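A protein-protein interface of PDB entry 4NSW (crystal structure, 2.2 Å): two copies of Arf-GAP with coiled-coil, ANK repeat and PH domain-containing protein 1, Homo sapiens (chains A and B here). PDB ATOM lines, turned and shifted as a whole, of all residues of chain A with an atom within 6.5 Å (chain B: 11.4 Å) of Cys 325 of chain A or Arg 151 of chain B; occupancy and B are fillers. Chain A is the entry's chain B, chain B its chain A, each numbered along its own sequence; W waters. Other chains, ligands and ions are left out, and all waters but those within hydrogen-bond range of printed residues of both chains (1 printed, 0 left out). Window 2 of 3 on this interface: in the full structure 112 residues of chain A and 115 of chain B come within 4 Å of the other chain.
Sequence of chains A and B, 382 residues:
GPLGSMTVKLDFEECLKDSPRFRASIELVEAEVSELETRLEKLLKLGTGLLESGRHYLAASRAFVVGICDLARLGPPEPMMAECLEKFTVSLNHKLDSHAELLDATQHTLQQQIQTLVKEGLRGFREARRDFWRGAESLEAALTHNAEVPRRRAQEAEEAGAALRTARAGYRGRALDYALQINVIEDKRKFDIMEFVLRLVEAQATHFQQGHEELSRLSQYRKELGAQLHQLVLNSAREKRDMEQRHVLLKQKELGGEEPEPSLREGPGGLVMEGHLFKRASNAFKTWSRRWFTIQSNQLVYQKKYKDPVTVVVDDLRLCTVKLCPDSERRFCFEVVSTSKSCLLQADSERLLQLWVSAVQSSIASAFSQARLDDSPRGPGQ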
ATOM      1  N   LYS A 323     -33.600   8.522  26.930  1.00  0.00           N
ATOM      2  CA  LYS A 323     -32.826   9.497  27.714  1.00  0.00           C
ATOM      3  C   LYS A 323     -31.344   9.152  27.779  1.00  0.00           C
ATOM      4  O   LYS A 323     -30.965   7.978  27.736  1.00  0.00           O
ATOM      5  CB  LYS A 323     -33.368   9.656  29.148  1.00  0.00           C
ATOM      6  CG  LYS A 323     -34.722   9.017  29.441  1.00  0.00           C
ATOM      7  CD  LYS A 323     -34.569   7.552  29.873  1.00  0.00           C
ATOM      8  CE  LYS A 323     -34.142   7.426  31.337  1.00  0.00           C
ATOM      9  NZ  LYS A 323     -35.180   7.900  32.306  1.00  0.00           N
ATOM     10  N   LEU A 324     -30.515  10.187  27.885  1.00  0.00           N
ATOM     11  CA  LEU A 324     -29.112  10.033  28.252  1.00  0.00           C
ATOM     12  C   LEU A 324     -29.028   9.465  29.672  1.00  0.00           C
ATOM     13  O   LEU A 324     -30.002   9.526  30.424  1.00  0.00           O
ATOM     14  CB  LEU A 324     -28.389  11.390  28.210  1.00  0.00           C
ATOM     15  CG  LEU A 324     -28.105  12.183  26.921  1.00  0.00           C
ATOM     16  CD1 LEU A 324     -27.485  11.299  25.813  1.00  0.00           C
ATOM     17  CD2 LEU A 324     -29.341  12.927  26.422  1.00  0.00           C
ATOM     18  N   CYS A 325     -27.875   8.908  30.030  1.00  0.00           N
ATOM     19  CA  CYS A 325     -27.617   8.496  31.411  1.00  0.00           C
ATOM     20  C   CYS A 325     -26.417   9.269  31.969  1.00  0.00           C
ATOM     21  O   CYS A 325     -25.281   8.784  31.894  1.00  0.00           O
ATOM     22  CB  CYS A 325     -27.361   6.988  31.513  1.00  0.00           C
ATOM     23  SG  CYS A 325     -28.572   5.913  30.694  1.00  0.00           S
ATOM     24  N   PRO A 326     -26.659  10.480  32.516  1.00  0.00           N
ATOM     25  CA  PRO A 326     -25.584  11.257  33.140  1.00  0.00           C
ATOM     26  C   PRO A 326     -25.172  10.646  34.483  1.00  0.00           C
ATOM     27  O   PRO A 326     -24.218  11.114  35.116  1.00  0.00           O
ATOM     28  CB  PRO A 326     -26.228  12.629  33.360  1.00  0.00           C
ATOM     29  CG  PRO A 326     -27.681  12.336  33.532  1.00  0.00           C
ATOM     30  CD  PRO A 326     -27.957  11.182  32.595  1.00  0.00           C
ATOM     31  N   ASP A 327     -25.907   9.614  34.899  1.00  0.00           N
ATOM     32  CA  ASP A 327     -25.646   8.903  36.145  1.00  0.00           C
ATOM     33  C   ASP A 327     -25.310   7.429  35.871  1.00  0.00           C
ATOM     34  O   ASP A 327     -25.711   6.542  36.632  1.00  0.00           O
ATOM     35  CB  ASP A 327     -26.846   9.032  37.095  1.00  0.00           C
ATOM     36  CG  ASP A 327     -26.432   9.138  38.569  1.00  0.00           C
ATOM     37  OD1 ASP A 327     -26.449  10.265  39.122  1.00  0.00           O
ATOM     38  OD2 ASP A 327     -26.096   8.093  39.175  1.00  0.00           O
ATOM     39  N   SER A 328     -24.604   7.171  34.766  1.00  0.00           N
ATOM     40  CA  SER A 328     -23.890   5.899  34.600  1.00  0.00           C
ATOM     41  C   SER A 328     -22.376   6.106  34.442  1.00  0.00           C
ATOM     42  O   SER A 328     -21.909   7.189  34.073  1.00  0.00           O
ATOM     43  CB  SER A 328     -24.489   5.006  33.493  1.00  0.00           C
ATOM     44  OG  SER A 328     -24.108   5.431  32.199  1.00  0.00           O
ATOM     45  N   GLU A 329     -21.628   5.050  34.747  1.00  0.00           N
ATOM     46  CA  GLU A 329     -20.166   5.078  34.811  1.00  0.00           C
ATOM     47  C   GLU A 329     -19.478   5.255  33.453  1.00  0.00           C
ATOM     48  O   GLU A 329     -18.540   6.052  33.308  1.00  0.00           O
ATOM     49  CB  GLU A 329     -19.652   3.808  35.504  1.00  0.00           C
ATOM     50  CG  GLU A 329     -20.251   2.499  34.965  1.00  0.00           C
ATOM     51  CD  GLU A 329     -20.144   1.354  35.945  1.00  0.00           C
ATOM     52  OE1 GLU A 329     -19.757   1.606  37.110  1.00  0.00           O
ATOM     53  OE2 GLU A 329     -20.453   0.199  35.553  1.00  0.00           O
ATOM     54  N   ARG A 330     -19.950   4.513  32.464  1.00  0.00           N
ATOM     55  CA  ARG A 330     -19.324   4.507  31.152  1.00  0.00           C
ATOM     56  C   ARG A 330     -19.933   5.559  30.243  1.00  0.00           C
ATOM     57  O   ARG A 330     -21.084   5.971  30.443  1.00  0.00           O
ATOM     58  CB  ARG A 330     -19.388   3.118  30.536  1.00  0.00           C
ATOM     59  CG  ARG A 330     -20.658   2.376  30.812  1.00  0.00           C
ATOM     60  CD  ARG A 330     -20.352   0.919  30.956  1.00  0.00           C
ATOM     61  NE  ARG A 330     -20.147   0.260  29.671  1.00  0.00           N
ATOM     62  CZ  ARG A 330     -19.311  -0.755  29.474  1.00  0.00           C
ATOM     63  NH1 ARG A 330     -18.585  -1.224  30.469  1.00  0.00           N
ATOM     64  NH2 ARG A 330     -19.204  -1.303  28.276  1.00  0.00           N
ATOM     65  N   ARG A 331     -19.139   6.005  29.268  1.00  0.00           N
ATOM     66  CA  ARG A 331     -19.532   7.089  28.380  1.00  0.00           C
ATOM     67  C   ARG A 331     -20.460   6.603  27.291  1.00  0.00           C
ATOM     68  O   ARG A 331     -20.431   5.432  26.924  1.00  0.00           O
ATOM     69  CB  ARG A 331     -18.312   7.731  27.710  1.00  0.00           C
ATOM     70  CG  ARG A 331     -17.302   8.405  28.639  1.00  0.00           C
ATOM     71  CD  ARG A 331     -16.042   8.723  27.838  1.00  0.00           C
ATOM     72  NE  ARG A 331     -15.545   7.506  27.204  1.00  0.00           N
ATOM     73  CZ  ARG A 331     -14.840   7.453  26.081  1.00  0.00           C
ATOM     74  NH1 ARG A 331     -14.518   8.564  25.426  1.00  0.00           N
ATOM     75  NH2 ARG A 331     -14.466   6.265  25.607  1.00  0.00           N
ATOM     76  N   PHE A 332     -21.261   7.535  26.781  1.00  0.00           N
ATOM     77  CA  PHE A 332     -22.099   7.364  25.587  1.00  0.00           C
ATOM     78  C   PHE A 332     -23.285   6.449  25.835  1.00  0.00           C
ATOM     79  O   PHE A 332     -23.784   5.801  24.918  1.00  0.00           O
ATOM     80  CB  PHE A 332     -21.268   6.925  24.359  1.00  0.00           C
ATOM     81  CG  PHE A 332     -19.996   7.716  24.172  1.00  0.00           C
ATOM     82  CD1 PHE A 332     -20.027   9.105  24.054  1.00  0.00           C
ATOM     83  CD2 PHE A 332     -18.763   7.073  24.135  1.00  0.00           C
ATOM     84  CE1 PHE A 332     -18.842   9.849  23.901  1.00  0.00           C
ATOM     85  CE2 PHE A 332     -17.576   7.805  23.982  1.00  0.00           C
ATOM     86  CZ  PHE A 332     -17.617   9.196  23.865  1.00  0.00           C
ATOM     87  N   CYS A 333     -23.738   6.416  27.084  1.00  0.00           N
ATOM     88  CA  CYS A 333     -24.880   5.597  27.472  1.00  0.00           C
ATOM     89  C   CYS A 333     -26.240   6.243  27.225  1.00  0.00           C
ATOM     90  O   CYS A 333     -26.416   7.452  27.370  1.00  0.00           O
ATOM     91  CB  CYS A 333     -24.769   5.201  28.939  1.00  0.00           C
ATOM     92  SG  CYS A 333     -23.665   3.836  29.129  1.00  0.00           S
ATOM     93  N   PHE A 334     -27.204   5.404  26.870  1.00  0.00           N
ATOM     94  CA  PHE A 334     -28.583   5.831  26.766  1.00  0.00           C
ATOM     95  C   PHE A 334     -29.530   4.700  27.094  1.00  0.00           C
ATOM     96  O   PHE A 334     -29.164   3.527  27.056  1.00  0.00           O
ATOM     97  CB  PHE A 334     -28.901   6.470  25.404  1.00  0.00           C
ATOM     98  CG  PHE A 334     -28.686   5.574  24.213  1.00  0.00           C
ATOM     99  CD1 PHE A 334     -29.776   5.112  23.475  1.00  0.00           C
ATOM    100  CD2 PHE A 334     -27.398   5.235  23.788  1.00  0.00           C
ATOM    101  CE1 PHE A 334     -29.591   4.307  22.352  1.00  0.00           C
ATOM    102  CE2 PHE A 334     -27.200   4.431  22.665  1.00  0.00           C
ATOM    103  CZ  PHE A 334     -28.296   3.959  21.948  1.00  0.00           C
ATOM    104  N   GLU A 335     -30.757   5.076  27.418  1.00  0.00           N
ATOM    105  CA  GLU A 335     -31.758   4.134  27.837  1.00  0.00           C
ATOM    106  C   GLU A 335     -33.010   4.273  26.987  1.00  0.00           C
ATOM    107  O   GLU A 335     -33.448   5.379  26.675  1.00  0.00           O
ATOM    108  CB  GLU A 335     -32.087   4.376  29.306  1.00  0.00           C
ATOM    109  CG  GLU A 335     -33.054   3.375  29.898  1.00  0.00           C
ATOM    110  CD  GLU A 335     -33.006   3.341  31.415  1.00  0.00           C
ATOM    111  OE1 GLU A 335     -32.650   2.267  31.964  1.00  0.00           O
ATOM    112  OE2 GLU A 335     -33.305   4.380  32.049  1.00  0.00           O
ATOM    113  N   LEU A 344     -30.720  -0.772  28.631  1.00  0.00           N
ATOM    114  CA  LEU A 344     -29.548   0.099  28.611  1.00  0.00           C
ATOM    115  C   LEU A 344     -28.606  -0.179  27.428  1.00  0.00           C
ATOM    116  O   LEU A 344     -28.230  -1.313  27.190  1.00  0.00           O
ATOM    117  CB  LEU A 344     -28.768  -0.065  29.913  1.00  0.00           C
ATOM    118  CG  LEU A 344     -29.164   0.754  31.126  1.00  0.00           C
ATOM    119  CD1 LEU A 344     -30.269   0.074  31.981  1.00  0.00           C
ATOM    120  CD2 LEU A 344     -27.902   0.976  31.943  1.00  0.00           C
ATOM    121  N   LEU A 345     -28.209   0.871  26.717  1.00  0.00           N
ATOM    122  CA  LEU A 345     -27.379   0.752  25.504  1.00  0.00           C
ATOM    123  C   LEU A 345     -26.246   1.756  25.530  1.00  0.00           C
ATOM    124  O   LEU A 345     -26.294   2.742  26.257  1.00  0.00           O
ATOM    125  CB  LEU A 345     -28.218   0.978  24.244  1.00  0.00           C
ATOM    126  CG  LEU A 345     -29.544   0.229  24.099  1.00  0.00           C
ATOM    127  CD1 LEU A 345     -30.381   0.846  22.994  1.00  0.00           C
ATOM    128  CD2 LEU A 345     -29.292  -1.247  23.846  1.00  0.00           C
ATOM    129  N   HIS B 145     -12.444  -1.880  25.337  1.00  0.00           N
ATOM    130  CA  HIS B 145     -11.576  -0.972  26.074  1.00  0.00           C
ATOM    131  C   HIS B 145     -12.103   0.431  25.994  1.00  0.00           C
ATOM    132  O   HIS B 145     -12.166   1.127  27.011  1.00  0.00           O
ATOM    133  CB  HIS B 145     -10.127  -1.010  25.573  1.00  0.00           C
ATOM    134  CG  HIS B 145      -9.209  -0.133  26.366  1.00  0.00           C
ATOM    135  ND1 HIS B 145      -8.818  -0.443  27.655  1.00  0.00           N
ATOM    136  CD2 HIS B 145      -8.646   1.066  26.076  1.00  0.00           C
ATOM    137  CE1 HIS B 145      -8.042   0.522  28.118  1.00  0.00           C
ATOM    138  NE2 HIS B 145      -7.925   1.450  27.181  1.00  0.00           N
ATOM    139  N   ASN B 146     -12.478   0.845  24.783  1.00  0.00           N
ATOM    140  CA  ASN B 146     -13.101   2.138  24.560  1.00  0.00           C
ATOM    141  C   ASN B 146     -14.377   2.307  25.369  1.00  0.00           C
ATOM    142  O   ASN B 146     -14.528   3.279  26.118  1.00  0.00           O
ATOM    143  CB  ASN B 146     -13.391   2.352  23.079  1.00  0.00           C
ATOM    144  CG  ASN B 146     -13.902   3.756  22.777  1.00  0.00           C
ATOM    145  OD1 ASN B 146     -14.989   3.917  22.202  1.00  0.00           O
ATOM    146  ND2 ASN B 146     -13.115   4.789  23.162  1.00  0.00           N
ATOM    147  N   ALA B 147     -15.285   1.345  25.230  1.00  0.00           N
ATOM    148  CA  ALA B 147     -16.570   1.383  25.912  1.00  0.00           C
ATOM    149  C   ALA B 147     -16.425   1.447  27.444  1.00  0.00           C
ATOM    150  O   ALA B 147     -17.316   1.944  28.129  1.00  0.00           O
ATOM    151  CB  ALA B 147     -17.404   0.167  25.503  1.00  0.00           C
ATOM    152  N   GLU B 148     -15.317   0.910  27.968  1.00  0.00           N
ATOM    153  CA  GLU B 148     -15.057   0.827  29.415  1.00  0.00           C
ATOM    154  C   GLU B 148     -14.344   2.037  30.044  1.00  0.00           C
ATOM    155  O   GLU B 148     -14.305   2.147  31.262  1.00  0.00           O
ATOM    156  CB  GLU B 148     -14.254  -0.432  29.736  1.00  0.00           C
ATOM    157  CG  GLU B 148     -15.101  -1.662  29.976  1.00  0.00           C
ATOM    158  CD  GLU B 148     -14.294  -2.941  29.911  1.00  0.00           C
ATOM    159  OE1 GLU B 148     -13.096  -2.863  29.563  1.00  0.00           O
ATOM    160  OE2 GLU B 148     -14.846  -4.033  30.196  1.00  0.00           O
ATOM    161  N   VAL B 149     -13.755   2.929  29.243  1.00  0.00           N
ATOM    162  CA  VAL B 149     -13.026   4.045  29.865  1.00  0.00           C
ATOM    163  C   VAL B 149     -13.956   5.047  30.568  1.00  0.00           C
ATOM    164  O   VAL B 149     -14.980   5.454  30.009  1.00  0.00           O
ATOM    165  CB  VAL B 149     -11.911   4.689  28.982  1.00  0.00           C
ATOM    166  CG1 VAL B 149     -10.700   3.751  28.914  1.00  0.00           C
ATOM    167  CG2 VAL B 149     -12.395   5.051  27.572  1.00  0.00           C
ATOM    168  N   PRO B 150     -13.614   5.385  31.828  1.00  0.00           N
ATOM    169  CA  PRO B 150     -14.419   6.160  32.760  1.00  0.00           C
ATOM    170  C   PRO B 150     -14.820   7.543  32.309  1.00  0.00           C
ATOM    171  O   PRO B 150     -14.153   8.161  31.475  1.00  0.00           O
ATOM    172  CB  PRO B 150     -13.520   6.252  33.988  1.00  0.00           C
ATOM    173  CG  PRO B 150     -12.761   4.972  33.946  1.00  0.00           C
ATOM    174  CD  PRO B 150     -12.420   4.839  32.501  1.00  0.00           C
ATOM    175  N   ARG B 151     -15.921   7.990  32.908  1.00  0.00           N
ATOM    176  CA  ARG B 151     -16.599   9.254  32.653  1.00  0.00           C
ATOM    177  C   ARG B 151     -15.649  10.412  32.382  1.00  0.00           C
ATOM    178  O   ARG B 151     -15.479  10.808  31.226  1.00  0.00           O
ATOM    179  CB  ARG B 151     -17.531   9.567  33.832  1.00  0.00           C
ATOM    180  CG  ARG B 151     -18.440  10.783  33.668  1.00  0.00           C
ATOM    181  CD  ARG B 151     -19.759  10.409  33.014  1.00  0.00           C
ATOM    182  NE  ARG B 151     -19.702  10.498  31.556  1.00  0.00           N
ATOM    183  CZ  ARG B 151     -20.674  10.082  30.747  1.00  0.00           C
ATOM    184  NH1 ARG B 151     -21.778   9.542  31.253  1.00  0.00           N
ATOM    185  NH2 ARG B 151     -20.540  10.205  29.432  1.00  0.00           N
ATOM    186  N   ARG B 152     -15.024  10.946  33.432  1.00  0.00           N
ATOM    187  CA  ARG B 152     -14.178  12.140  33.278  1.00  0.00           C
ATOM    188  C   ARG B 152     -12.664  11.852  33.230  1.00  0.00           C
ATOM    189  O   ARG B 152     -11.859  12.610  33.775  1.00  0.00           O
ATOM    190  CB  ARG B 152     -14.539  13.218  34.319  1.00  0.00           C
ATOM    191  CG  ARG B 152     -16.042  13.600  34.407  1.00  0.00           C
ATOM    192  CD  ARG B 152     -16.587  14.257  33.125  1.00  0.00           C
ATOM    193  NE  ARG B 152     -16.890  13.277  32.078  1.00  0.00           N
ATOM    194  CZ  ARG B 152     -17.368  13.558  30.862  1.00  0.00           C
ATOM    195  NH1 ARG B 152     -17.602  12.564  30.009  1.00  0.00           N
ATOM    196  NH2 ARG B 152     -17.623  14.812  30.498  1.00  0.00           N
ATOM    197  N   ARG B 153     -12.295  10.752  32.569  1.00  0.00           N
ATOM    198  CA  ARG B 153     -10.896  10.463  32.228  1.00  0.00           C
ATOM    199  C   ARG B 153     -10.599  10.898  30.792  1.00  0.00           C
ATOM    200  O   ARG B 153     -10.270  10.069  29.936  1.00  0.00           O
ATOM    201  CB  ARG B 153     -10.555   8.977  32.452  1.00  0.00           C
ATOM    202  CG  ARG B 153      -9.893   8.673  33.802  1.00  0.00           C
ATOM    203  CD  ARG B 153     -10.113   7.228  34.217  1.00  0.00           C
ATOM    204  NE  ARG B 153      -9.956   6.971  35.655  1.00  0.00           N
ATOM    205  CZ  ARG B 153     -10.780   7.403  36.614  1.00  0.00           C
ATOM    206  NH1 ARG B 153     -10.539   7.090  37.883  1.00  0.00           N
ATOM    207  NH2 ARG B 153     -11.835   8.162  36.323  1.00  0.00           N
ATOM    208  N   ALA B 154     -10.712  12.208  30.542  1.00  0.00           N
ATOM    209  CA  ALA B 154     -10.585  12.786  29.185  1.00  0.00           C
ATOM    210  C   ALA B 154      -9.290  12.407  28.441  1.00  0.00           C
ATOM    211  O   ALA B 154      -9.280  12.309  27.207  1.00  0.00           O
ATOM    212  CB  ALA B 154     -10.755  14.296  29.226  1.00  0.00           C
ATOM    213  N   GLN B 155      -8.222  12.207  29.219  1.00  0.00           N
ATOM    214  CA  GLN B 155      -6.934  11.703  28.747  1.00  0.00           C
ATOM    215  C   GLN B 155      -7.015  10.235  28.294  1.00  0.00           C
ATOM    216  O   GLN B 155      -6.622   9.911  27.177  1.00  0.00           O
ATOM    217  CB  GLN B 155      -5.845  11.911  29.829  1.00  0.00           C
ATOM    218  CG  GLN B 155      -4.608  10.971  29.766  1.00  0.00           C
ATOM    219  CD  GLN B 155      -3.765  11.136  28.499  1.00  0.00           C
ATOM    220  OE1 GLN B 155      -3.968  12.067  27.713  1.00  0.00           O
ATOM    221  NE2 GLN B 155      -2.816  10.222  28.296  1.00  0.00           N
ATOM    222  N   GLU B 156      -7.510   9.350  29.156  1.00  0.00           N
ATOM    223  CA  GLU B 156      -7.658   7.948  28.773  1.00  0.00           C
ATOM    224  C   GLU B 156      -8.663   7.756  27.633  1.00  0.00           C
ATOM    225  O   GLU B 156      -8.502   6.870  26.804  1.00  0.00           O
ATOM    226  CB  GLU B 156      -7.992   7.070  29.978  1.00  0.00           C
ATOM    227  CG  GLU B 156      -6.766   6.361  30.542  1.00  0.00           C
ATOM    228  CD  GLU B 156      -7.102   5.075  31.276  1.00  0.00           C
ATOM    229  OE1 GLU B 156      -6.776   4.990  32.484  1.00  0.00           O
ATOM    230  OE2 GLU B 156      -7.688   4.150  30.653  1.00  0.00           O
ATOM    231  N   ALA B 157      -9.683   8.607  27.603  1.00  0.00           N
ATOM    232  CA  ALA B 157     -10.613   8.697  26.491  1.00  0.00           C
ATOM    233  C   ALA B 157      -9.869   9.025  25.202  1.00  0.00           C
ATOM    234  O   ALA B 157     -10.117   8.394  24.170  1.00  0.00           O
ATOM    235  CB  ALA B 157     -11.678   9.752  26.775  1.00  0.00           C
ATOM    236  N   GLU B 158      -8.965  10.010  25.271  1.00  0.00           N
ATOM    237  CA  GLU B 158      -8.048  10.320  24.167  1.00  0.00           C
ATOM    238  C   GLU B 158      -7.331   9.073  23.641  1.00  0.00           C
ATOM    239  O   GLU B 158      -7.394   8.779  22.451  1.00  0.00           O
ATOM    240  CB  GLU B 158      -7.005  11.379  24.581  1.00  0.00           C
ATOM    241  CG  GLU B 158      -7.276  12.790  24.095  1.00  0.00           C
ATOM    242  CD  GLU B 158      -6.820  13.046  22.660  1.00  0.00           C
ATOM    243  OE1 GLU B 158      -6.621  14.234  22.327  1.00  0.00           O
ATOM    244  OE2 GLU B 158      -6.663  12.088  21.862  1.00  0.00           O
ATOM    245  N   GLU B 159      -6.663   8.350  24.538  1.00  0.00           N
ATOM    246  CA  GLU B 159      -5.889   7.173  24.165  1.00  0.00           C
ATOM    247  C   GLU B 159      -6.717   5.982  23.687  1.00  0.00           C
ATOM    248  O   GLU B 159      -6.352   5.339  22.700  1.00  0.00           O
ATOM    249  CB  GLU B 159      -4.955   6.748  25.303  1.00  0.00           C
ATOM    250  CG  GLU B 159      -3.706   7.620  25.394  1.00  0.00           C
ATOM    251  CD  GLU B 159      -2.715   7.145  26.450  1.00  0.00           C
ATOM    252  OE1 GLU B 159      -3.039   7.239  27.657  1.00  0.00           O
ATOM    253  OE2 GLU B 159      -1.602   6.699  26.070  1.00  0.00           O
ATOM    254  N   ALA B 160      -7.805   5.662  24.383  1.00  0.00           N
ATOM    255  CA  ALA B 160      -8.671   4.566  23.929  1.00  0.00           C
ATOM    256  C   ALA B 160      -9.177   4.855  22.507  1.00  0.00           C
ATOM    257  O   ALA B 160      -9.186   3.962  21.658  1.00  0.00           O
ATOM    258  CB  ALA B 160      -9.818   4.352  24.869  1.00  0.00           C
HETATM  259  O   HOH W   1     -23.328   8.018  29.668  1.00  0.00           O
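N of Arg 151 of chain B is in hydrogen-bond range of O of Glu 329 of chain A (3.3 Å). The backbone carbonyl oxygen (O) of Asn 146 of chain B lies within hydrogen-bond range of the guanidinium group (NH2) of Arg 331 of chain A (3.0 Å).
No position is printed for both chains.
N of Cys 325 of chain A is in hydrogen-bond range of O of Cys 333 of chain A (3.4 Å). OG of Ser 328 of chain A sits close to SG of Cys 333 of chain A. The backbone carbonyl oxygen of Arg 330 of chain A lies within hydrogen-bond range of the side-chain sulfur of Cys 333 of chain A (3.6 Å).
Arg 151 of chain B touches Cys 325 of chain A. Arg 151 of chain B touches Ser 328 of chain A (NH1 to O, 3.7 Å). Arg 330 of chain A touches Ala 147 of chain B. CG of Glu 148 of chain B touches NH1 of Arg 330 of chain A, at 3.5 Å. Arg 330 of chain A touches Arg 151 of chain B. NH2 of Arg 331 of chain A touches CG2 of Val 149 of chain B (3.1 Å). Arg 151 of chain B touches Arg 331 of chain A (NH2 to CA, 3.4 Å). NH1 of Arg 331 of chain A touches CB of Ala 157 of chain B, 3.4 Å away. Phe 332 of chain A touches Arg 151 of chain B (N to NH2, 3.8 Å).
Water W1 lies within hydrogen-bond range of NH1 of Arg 151 of chain B (2.7 Å), O of Cys 325 of chain A (3.1 Å), N of Cys 333 of chain A (3.1 Å) and O of Arg 330 of chain A (3.1 Å).
Cys 325 of chain A touches just one residue of chain B: Arg 151. Arg 151 of chain B touches six residues of chain A. No residue of chain B comes within 4 Å of Lys 323 of chain A. No residue of chain B comes within 4 Å of Leu 324 of chain A. Pro 326 of chain A touches none of the printed residues of chain B. Ser 328 of chain A touches just one residue of chain B: Arg 151 (3.7 Å). Arg 331 of chain A touches four residues of chain B. Of chain B, only Arg 151 (3.8 Å) comes within 4 Å of Phe 332 of chain A. Of the printed residues of chain B, Glu 329 of chain A touches Arg 151. Of the printed residues of chain A, Val 149 of chain B touches Arg 331 (3.1 Å). The nearest residue of chain A that does not touch Arg 151 of chain B is Pro 326 of chain A (4.6 Å). The nearest printed residue of chain A that does not touch Ala 157 of chain B is Phe 332 of chain A (6.6 Å).
Of the 15 printed residues of chain A, 6 touch a printed residue of chain B. Of the 16 printed residues of chain B, 6 touch a printed residue of chain A. Hydrophobic or aromatic side chains of chain B that line the printed part of chain A: Ala 147, Val 149 and Ala 157. Among the printed residues, no Asp or Glu carboxylate lies within 4 Å of a Lys or Arg side-chain nitrogen of the other chain.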
